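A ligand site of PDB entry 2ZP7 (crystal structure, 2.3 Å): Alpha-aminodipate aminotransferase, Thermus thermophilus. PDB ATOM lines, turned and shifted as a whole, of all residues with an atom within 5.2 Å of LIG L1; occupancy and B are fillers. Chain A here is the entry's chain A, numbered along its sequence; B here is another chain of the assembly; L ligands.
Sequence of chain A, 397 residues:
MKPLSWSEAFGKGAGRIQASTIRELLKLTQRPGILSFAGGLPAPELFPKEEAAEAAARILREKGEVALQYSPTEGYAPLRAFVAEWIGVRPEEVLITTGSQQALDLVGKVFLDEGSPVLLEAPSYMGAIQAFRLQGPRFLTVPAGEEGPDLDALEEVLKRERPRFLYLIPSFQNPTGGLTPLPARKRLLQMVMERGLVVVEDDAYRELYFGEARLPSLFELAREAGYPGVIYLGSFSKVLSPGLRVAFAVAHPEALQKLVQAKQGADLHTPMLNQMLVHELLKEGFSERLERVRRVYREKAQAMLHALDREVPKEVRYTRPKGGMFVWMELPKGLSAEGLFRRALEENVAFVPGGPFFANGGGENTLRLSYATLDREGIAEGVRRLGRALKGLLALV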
ATOM      1  N   THR A  98     -17.567  28.837  -4.419  1.00  0.00           N
ATOM      2  CA  THR A  98     -18.836  29.227  -3.835  1.00  0.00           C
ATOM      3  C   THR A  98     -18.771  28.966  -2.331  1.00  0.00           C
ATOM      4  O   THR A  98     -19.359  27.993  -1.814  1.00  0.00           O
ATOM      5  CB  THR A  98     -20.034  28.479  -4.515  1.00  0.00           C
ATOM      6  OG1 THR A  98     -19.905  28.561  -5.949  1.00  0.00           O
ATOM      7  CG2 THR A  98     -21.381  29.054  -4.076  1.00  0.00           C
ATOM      8  N   GLY A  99     -18.033  29.860  -1.649  1.00  0.00           N
ATOM      9  CA  GLY A  99     -17.614  29.715  -0.251  1.00  0.00           C
ATOM     10  C   GLY A  99     -16.407  28.787  -0.163  1.00  0.00           C
ATOM     11  O   GLY A  99     -16.096  28.082  -1.105  1.00  0.00           O
ATOM     12  N   SER A 100     -15.699  28.818   0.972  1.00  0.00           N
ATOM     13  CA  SER A 100     -14.644  27.836   1.264  1.00  0.00           C
ATOM     14  C   SER A 100     -15.209  26.437   1.518  1.00  0.00           C
ATOM     15  O   SER A 100     -14.505  25.443   1.393  1.00  0.00           O
ATOM     16  CB  SER A 100     -13.859  28.253   2.520  1.00  0.00           C
ATOM     17  OG  SER A 100     -12.894  29.223   2.209  1.00  0.00           O
ATOM     18  N   GLN A 101     -16.493  26.370   1.872  1.00  0.00           N
ATOM     19  CA  GLN A 101     -17.156  25.085   1.988  1.00  0.00           C
ATOM     20  C   GLN A 101     -17.091  24.282   0.690  1.00  0.00           C
ATOM     21  O   GLN A 101     -16.835  23.080   0.718  1.00  0.00           O
ATOM     22  CB  GLN A 101     -18.592  25.255   2.455  1.00  0.00           C
ATOM     23  CG  GLN A 101     -19.326  23.935   2.703  1.00  0.00           C
ATOM     24  CD  GLN A 101     -18.651  23.119   3.774  1.00  0.00           C
ATOM     25  OE1 GLN A 101     -18.282  21.953   3.561  1.00  0.00           O
ATOM     26  NE2 GLN A 101     -18.485  23.728   4.921  1.00  0.00           N
ATOM     27  N   GLN A 102     -17.317  24.928  -0.460  1.00  0.00           N
ATOM     28  CA  GLN A 102     -17.194  24.244  -1.764  1.00  0.00           C
ATOM     29  C   GLN A 102     -15.765  23.717  -1.971  1.00  0.00           C
ATOM     30  O   GLN A 102     -15.553  22.580  -2.417  1.00  0.00           O
ATOM     31  CB  GLN A 102     -17.573  25.173  -2.907  1.00  0.00           C
ATOM     32  CG  GLN A 102     -17.206  24.604  -4.264  1.00  0.00           C
ATOM     33  CD  GLN A 102     -17.794  25.385  -5.404  1.00  0.00           C
ATOM     34  OE1 GLN A 102     -17.291  26.453  -5.769  1.00  0.00           O
ATOM     35  NE2 GLN A 102     -18.872  24.872  -5.975  1.00  0.00           N
ATOM     36  N   LEU A 104     -13.546  22.912   0.286  1.00  0.00           N
ATOM     37  CA  LEU A 104     -13.438  21.686   1.081  1.00  0.00           C
ATOM     38  C   LEU A 104     -14.055  20.445   0.397  1.00  0.00           C
ATOM     39  O   LEU A 104     -13.475  19.353   0.430  1.00  0.00           O
ATOM     40  CB  LEU A 104     -14.090  21.908   2.459  1.00  0.00           C
ATOM     41  CG  LEU A 104     -13.446  23.012   3.333  1.00  0.00           C
ATOM     42  CD1 LEU A 104     -14.300  23.341   4.562  1.00  0.00           C
ATOM     43  CD2 LEU A 104     -12.069  22.575   3.716  1.00  0.00           C
ATOM     44  N   TYR A 125     -12.842  21.706  12.216  1.00  0.00           N
ATOM     45  CA  TYR A 125     -13.997  22.368  11.656  1.00  0.00           C
ATOM     46  C   TYR A 125     -15.062  21.386  11.122  1.00  0.00           C
ATOM     47  O   TYR A 125     -14.777  20.521  10.301  1.00  0.00           O
ATOM     48  CB  TYR A 125     -13.572  23.444  10.633  1.00  0.00           C
ATOM     49  CG  TYR A 125     -14.712  24.056   9.866  1.00  0.00           C
ATOM     50  CD1 TYR A 125     -15.820  24.566  10.524  1.00  0.00           C
ATOM     51  CD2 TYR A 125     -14.676  24.114   8.473  1.00  0.00           C
ATOM     52  CE1 TYR A 125     -16.884  25.119   9.827  1.00  0.00           C
ATOM     53  CE2 TYR A 125     -15.730  24.662   7.757  1.00  0.00           C
ATOM     54  CZ  TYR A 125     -16.823  25.165   8.440  1.00  0.00           C
ATOM     55  OH  TYR A 125     -17.884  25.705   7.737  1.00  0.00           O
ATOM     56  N   TYR A 167      -5.363  18.555   7.083  1.00  0.00           N
ATOM     57  CA  TYR A 167      -6.245  19.698   7.108  1.00  0.00           C
ATOM     58  C   TYR A 167      -6.026  20.527   8.381  1.00  0.00           C
ATOM     59  O   TYR A 167      -6.199  20.018   9.495  1.00  0.00           O
ATOM     60  CB  TYR A 167      -7.710  19.280   6.922  1.00  0.00           C
ATOM     61  CG  TYR A 167      -8.661  20.431   7.126  1.00  0.00           C
ATOM     62  CD1 TYR A 167      -8.871  21.364   6.127  1.00  0.00           C
ATOM     63  CD2 TYR A 167      -9.311  20.595   8.344  1.00  0.00           C
ATOM     64  CE1 TYR A 167      -9.738  22.442   6.332  1.00  0.00           C
ATOM     65  CE2 TYR A 167     -10.169  21.679   8.557  1.00  0.00           C
ATOM     66  CZ  TYR A 167     -10.375  22.596   7.544  1.00  0.00           C
ATOM     67  OH  TYR A 167     -11.217  23.661   7.754  1.00  0.00           O
ATOM     68  N   ILE A 169      -5.964  24.631  10.367  1.00  0.00           N
ATOM     69  CA  ILE A 169      -6.427  26.020  10.483  1.00  0.00           C
ATOM     70  C   ILE A 169      -5.481  26.705  11.499  1.00  0.00           C
ATOM     71  O   ILE A 169      -5.850  26.920  12.647  1.00  0.00           O
ATOM     72  CB  ILE A 169      -7.889  26.085  11.016  1.00  0.00           C
ATOM     73  CG1 ILE A 169      -8.838  25.185  10.189  1.00  0.00           C
ATOM     74  CG2 ILE A 169      -8.412  27.494  11.013  1.00  0.00           C
ATOM     75  CD1 ILE A 169     -10.063  24.722  10.952  1.00  0.00           C
ATOM     76  N   ASN A 174     -11.218  26.908  14.069  1.00  0.00           N
ATOM     77  CA  ASN A 174     -12.605  26.602  14.370  1.00  0.00           C
ATOM     78  C   ASN A 174     -12.608  25.145  14.848  1.00  0.00           C
ATOM     79  O   ASN A 174     -12.239  24.255  14.062  1.00  0.00           O
ATOM     80  CB  ASN A 174     -13.467  26.770  13.103  1.00  0.00           C
ATOM     81  CG  ASN A 174     -14.976  26.844  13.403  1.00  0.00           C
ATOM     82  OD1 ASN A 174     -15.414  26.478  14.471  1.00  0.00           O
ATOM     83  ND2 ASN A 174     -15.756  27.335  12.425  1.00  0.00           N
ATOM     84  N   ASP A 202      -6.709  26.099   5.780  1.00  0.00           N
ATOM     85  CA  ASP A 202      -7.911  26.885   5.752  1.00  0.00           C
ATOM     86  C   ASP A 202      -7.664  28.180   6.556  1.00  0.00           C
ATOM     87  O   ASP A 202      -7.465  28.152   7.758  1.00  0.00           O
ATOM     88  CB  ASP A 202      -9.040  26.026   6.316  1.00  0.00           C
ATOM     89  CG  ASP A 202     -10.385  26.639   6.131  1.00  0.00           C
ATOM     90  OD1 ASP A 202     -10.477  27.867   5.933  1.00  0.00           O
ATOM     91  OD2 ASP A 202     -11.368  25.871   6.214  1.00  0.00           O
ATOM     92  N   ALA A 204      -9.694  31.007   6.771  1.00  0.00           N
ATOM     93  CA  ALA A 204     -10.905  31.828   6.859  1.00  0.00           C
ATOM     94  C   ALA A 204     -10.786  33.009   7.838  1.00  0.00           C
ATOM     95  O   ALA A 204     -11.350  34.088   7.605  1.00  0.00           O
ATOM     96  CB  ALA A 204     -12.094  30.992   7.205  1.00  0.00           C
ATOM     97  N   TYR A 205     -10.042  32.822   8.915  1.00  0.00           N
ATOM     98  CA  TYR A 205      -9.907  33.856   9.935  1.00  0.00           C
ATOM     99  C   TYR A 205      -8.637  34.706   9.824  1.00  0.00           C
ATOM    100  O   TYR A 205      -8.383  35.533  10.696  1.00  0.00           O
ATOM    101  CB  TYR A 205     -10.034  33.205  11.317  1.00  0.00           C
ATOM    102  CG  TYR A 205     -11.355  32.502  11.441  1.00  0.00           C
ATOM    103  CD1 TYR A 205     -12.512  33.206  11.742  1.00  0.00           C
ATOM    104  CD2 TYR A 205     -11.449  31.144  11.167  1.00  0.00           C
ATOM    105  CE1 TYR A 205     -13.714  32.585  11.834  1.00  0.00           C
ATOM    106  CE2 TYR A 205     -12.667  30.498  11.236  1.00  0.00           C
ATOM    107  CZ  TYR A 205     -13.796  31.222  11.563  1.00  0.00           C
ATOM    108  OH  TYR A 205     -15.010  30.600  11.633  1.00  0.00           O
ATOM    109  N   SER A 235     -11.487  33.068   2.199  1.00  0.00           N
ATOM    110  CA  SER A 235     -12.914  33.357   2.039  1.00  0.00           C
ATOM    111  C   SER A 235     -13.213  34.838   2.294  1.00  0.00           C
ATOM    112  O   SER A 235     -12.506  35.466   3.045  1.00  0.00           O
ATOM    113  CB  SER A 235     -13.727  32.520   3.015  1.00  0.00           C
ATOM    114  OG  SER A 235     -15.107  32.701   2.805  1.00  0.00           O
ATOM    115  N   SER A 237     -16.114  35.549   3.602  1.00  0.00           N
ATOM    116  CA  SER A 237     -17.238  35.324   4.495  1.00  0.00           C
ATOM    117  C   SER A 237     -17.105  36.040   5.836  1.00  0.00           C
ATOM    118  O   SER A 237     -18.053  36.648   6.281  1.00  0.00           O
ATOM    119  CB  SER A 237     -17.461  33.819   4.715  1.00  0.00           C
ATOM    120  OG  SER A 237     -18.128  33.228   3.624  1.00  0.00           O
ATOM    121  N   LYS A 238     -15.954  35.925   6.479  1.00  0.00           N
ATOM    122  CA  LYS A 238     -15.773  36.481   7.834  1.00  0.00           C
ATOM    123  C   LYS A 238     -15.278  37.925   7.766  1.00  0.00           C
ATOM    124  O   LYS A 238     -15.160  38.619   8.778  1.00  0.00           O
ATOM    125  CB  LYS A 238     -14.791  35.598   8.647  1.00  0.00           C
ATOM    126  CG  LYS A 238     -15.182  34.099   8.773  1.00  0.00           C
ATOM    127  CD  LYS A 238     -16.706  33.905   8.860  1.00  0.00           C
ATOM    128  CE  LYS A 238     -17.126  32.559   9.465  1.00  0.00           C
ATOM    129  NZ  LYS A 238     -16.615  31.212   8.778  1.00  0.00           N
ATOM    130  N   PRO A 242     -20.790  36.358   4.367  1.00  0.00           N
ATOM    131  CA  PRO A 242     -21.036  34.924   4.242  1.00  0.00           C
ATOM    132  C   PRO A 242     -22.096  34.624   3.201  1.00  0.00           C
ATOM    133  O   PRO A 242     -21.942  33.711   2.397  1.00  0.00           O
ATOM    134  CB  PRO A 242     -21.605  34.531   5.611  1.00  0.00           C
ATOM    135  CG  PRO A 242     -21.398  35.670   6.502  1.00  0.00           C
ATOM    136  CD  PRO A 242     -21.176  36.873   5.693  1.00  0.00           C
ATOM    137  N   ARG A 245     -21.400  34.005  -0.626  1.00  0.00           N
ATOM    138  CA  ARG A 245     -20.741  32.730  -0.970  1.00  0.00           C
ATOM    139  C   ARG A 245     -19.580  32.944  -1.944  1.00  0.00           C
ATOM    140  O   ARG A 245     -19.563  32.373  -3.038  1.00  0.00           O
ATOM    141  CB  ARG A 245     -21.724  31.675  -1.525  1.00  0.00           C
ATOM    142  CG  ARG A 245     -23.069  31.515  -0.785  1.00  0.00           C
ATOM    143  CD  ARG A 245     -22.914  31.151   0.700  1.00  0.00           C
ATOM    144  NE  ARG A 245     -22.091  29.977   0.937  1.00  0.00           N
ATOM    145  CZ  ARG A 245     -21.032  29.945   1.738  1.00  0.00           C
ATOM    146  NH1 ARG A 245     -20.654  31.032   2.405  1.00  0.00           N
ATOM    147  NH2 ARG A 245     -20.344  28.836   1.857  1.00  0.00           N
ATOM    148  N   ALA A 247     -15.351  32.770  -2.186  1.00  0.00           N
ATOM    149  CA  ALA A 247     -14.098  32.415  -1.546  1.00  0.00           C
ATOM    150  C   ALA A 247     -13.073  32.060  -2.598  1.00  0.00           C
ATOM    151  O   ALA A 247     -13.305  32.241  -3.789  1.00  0.00           O
ATOM    152  CB  ALA A 247     -14.307  31.243  -0.620  1.00  0.00           C
ATOM    153  N   PHE A 326     -14.249  32.669  18.196  1.00  0.00           N
ATOM    154  CA  PHE A 326     -14.690  31.610  19.113  1.00  0.00           C
ATOM    155  C   PHE A 326     -13.939  31.552  20.428  1.00  0.00           C
ATOM    156  O   PHE A 326     -12.722  31.774  20.484  1.00  0.00           O
ATOM    157  CB  PHE A 326     -14.667  30.219  18.433  1.00  0.00           C
ATOM    158  CG  PHE A 326     -15.324  30.190  17.081  1.00  0.00           C
ATOM    159  CD1 PHE A 326     -16.700  30.352  16.955  1.00  0.00           C
ATOM    160  CD2 PHE A 326     -14.568  30.013  15.936  1.00  0.00           C
ATOM    161  CE1 PHE A 326     -17.309  30.334  15.697  1.00  0.00           C
ATOM    162  CE2 PHE A 326     -15.177  29.995  14.679  1.00  0.00           C
ATOM    163  CZ  PHE A 326     -16.551  30.152  14.566  1.00  0.00           C
ATOM    164  N   TYR B  70     -25.207  34.379   6.279  1.00  0.00           N
ATOM    165  CA  TYR B  70     -25.483  32.950   6.293  1.00  0.00           C
ATOM    166  C   TYR B  70     -26.975  32.692   6.418  1.00  0.00           C
ATOM    167  O   TYR B  70     -27.684  33.420   7.091  1.00  0.00           O
ATOM    168  CB  TYR B  70     -24.778  32.246   7.468  1.00  0.00           C
ATOM    169  CG  TYR B  70     -23.323  31.942   7.232  1.00  0.00           C
ATOM    170  CD1 TYR B  70     -22.915  31.296   6.060  1.00  0.00           C
ATOM    171  CD2 TYR B  70     -22.351  32.266   8.184  1.00  0.00           C
ATOM    172  CE1 TYR B  70     -21.568  31.008   5.837  1.00  0.00           C
ATOM    173  CE2 TYR B  70     -20.985  31.984   7.959  1.00  0.00           C
ATOM    174  CZ  TYR B  70     -20.615  31.360   6.788  1.00  0.00           C
ATOM    175  OH  TYR B  70     -19.292  31.076   6.540  1.00  0.00           O
ATOM    176  N   LEU B 268     -22.784  24.961   1.799  1.00  0.00           N
ATOM    177  CA  LEU B 268     -23.597  25.481   2.938  1.00  0.00           C
ATOM    178  C   LEU B 268     -25.013  25.892   2.499  1.00  0.00           C
ATOM    179  O   LEU B 268     -26.012  25.355   2.995  1.00  0.00           O
ATOM    180  CB  LEU B 268     -22.891  26.654   3.686  1.00  0.00           C
ATOM    181  CG  LEU B 268     -21.540  26.406   4.369  1.00  0.00           C
ATOM    182  CD1 LEU B 268     -21.092  27.627   5.188  1.00  0.00           C
ATOM    183  CD2 LEU B 268     -21.620  25.142   5.273  1.00  0.00           C
HETATM  184  N1  LIG L   1     -13.190  27.115   7.193  1.00  0.00           N
HETATM  185  C1  LIG L   1     -13.337  27.517   8.497  1.00  0.00           C
HETATM  186  C2  LIG L   1     -12.332  27.059   9.510  1.00  0.00           C
HETATM  187  C3  LIG L   1     -14.402  28.322   8.856  1.00  0.00           C
HETATM  188  O1  LIG L   1     -14.772  28.451  10.172  1.00  0.00           O
HETATM  189  C4  LIG L   1     -15.308  28.696   7.859  1.00  0.00           C
HETATM  190  C5  LIG L   1     -16.377  29.706   8.250  1.00  0.00           C
HETATM  191  C6  LIG L   1     -15.139  28.282   6.539  1.00  0.00           C
HETATM  192  C7  LIG L   1     -14.061  27.483   6.211  1.00  0.00           C
HETATM  193  C8  LIG L   1     -16.353  28.128   5.639  1.00  0.00           C
HETATM  194  O2  LIG L   1     -16.689  29.435   5.206  1.00  0.00           O
HETATM  195  P1  LIG L   1     -17.426  29.675   3.825  1.00  0.00           P
HETATM  196  O3  LIG L   1     -17.911  28.466   3.087  1.00  0.00           O
HETATM  197  O4  LIG L   1     -16.498  30.457   2.897  1.00  0.00           O
HETATM  198  O5  LIG L   1     -18.569  30.606   4.193  1.00  0.00           O
HETATM  199  N1  LG2 L   2     -18.969  29.172   9.367  1.00  0.00           N
HETATM  200  C1  LG2 L   2     -20.125  28.800  10.234  1.00  0.00           C
HETATM  201  C2  LG2 L   2     -19.615  28.445  11.627  1.00  0.00           C
HETATM  202  O1  LG2 L   2     -18.625  27.748  11.785  1.00  0.00           O
HETATM  203  C3  LG2 L   2     -20.877  27.614   9.622  1.00  0.00           C
HETATM  204  C4  LG2 L   2     -22.412  27.528   9.597  1.00  0.00           C
HETATM  205  C5  LG2 L   2     -22.984  26.712  10.755  1.00  0.00           C
HETATM  206  C6  LG2 L   2     -22.802  26.856   8.318  1.00  0.00           C
HETATM  207  O2  LG2 L   2     -20.183  28.829  12.633  1.00  0.00           O
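O4 of LIG L1 lies within hydrogen-bond range of N of Ser 100 (2.7 Å). N1 of LG2 L2 sits close to NZ of Lys 238. O1 of LIG L1 lies within hydrogen-bond range of ND2 of Asn 174 (2.7 Å). The side-chain hydroxyl (OH) of Tyr 205 lies within hydrogen-bond range of an oxygen (O1) of LIG L1, at 2.6 Å. N of Gln 101 lies within hydrogen-bond range of O3 of LIG L1 (2.8 Å). O1 of LG2 L2 lies within hydrogen-bond range of ND2 of Asn 174. The side-chain carboxylate (OD2) of Asp 202 sits at hydrogen-bond distance from a nitrogen (N1) of LIG L1 (2.4 Å). The side-chain amino group (NZ) of Lys 238 is bonded to a carbon (C5) of LIG L1 (1.6 Å). O3 of LIG L1 lies within salt-bridge range of NH2 of Arg 245 (2.8 Å). O5 of LIG L1 sits at hydrogen-bond distance from OG of Ser 237, at 2.7 Å. A nitrogen (N1) of LG2 L2 sits at hydrogen-bond distance from the side-chain hydroxyl (OH) of Tyr 70 of chain B (3.4 Å). An oxygen (O4) of LIG L1 sits at hydrogen-bond distance from the side-chain hydroxyl of Ser 235. An oxygen (O5) of LIG L1 lies within hydrogen-bond range of the side-chain hydroxyl (OH) of Tyr 70 of chain B (2.5 Å).
The backbone NH (N) of Tyr 125 is in hydrogen-bond range of the backbone carbonyl oxygen (O) of Asn 174, 3.2 Å away. N of Gly 99 sits at hydrogen-bond distance from O of Arg 245. NE2 of Gln 101 lies within hydrogen-bond range of OH of Tyr 125, at 3.5 Å. NZ of Lys 238 lies within hydrogen-bond range of OH of Tyr 205, at 3.3 Å. The guanidinium group (NH1) of Arg 245 lies within hydrogen-bond range of the backbone carbonyl oxygen (O) of Pro 242 (3.0 Å). OH of Tyr 167 is in hydrogen-bond range of OD2 of Asp 202 (2.7 Å). OD1 of Asp 202 sits at hydrogen-bond distance from N of Ala 204, at 3.3 Å. The side-chain hydroxyl (OH) of Tyr 205 lies within hydrogen-bond range of the side-chain amide nitrogen (ND2) of Asn 174, 3.4 Å away.
Gly 99 touches LIG L1 (CA to O4, 3.4 Å). Tyr 125 touches LIG L1. OH of Tyr 167 touches C2 of LIG L1 (3.98 Å). Ile 169 touches LIG L1. Ala 204 touches LIG L1 (CB to C3, 3.9 Å). Leu 268 of chain B touches LIG L1. Of the 22 residues printed, 16 come within 4 Å of LIG L1. Along chain A the residues within 4 Å of LIG L1 span positions 99 to 245. The nearest printed residue that does not touch LIG L1 is Ala 247 (4.2 Å).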
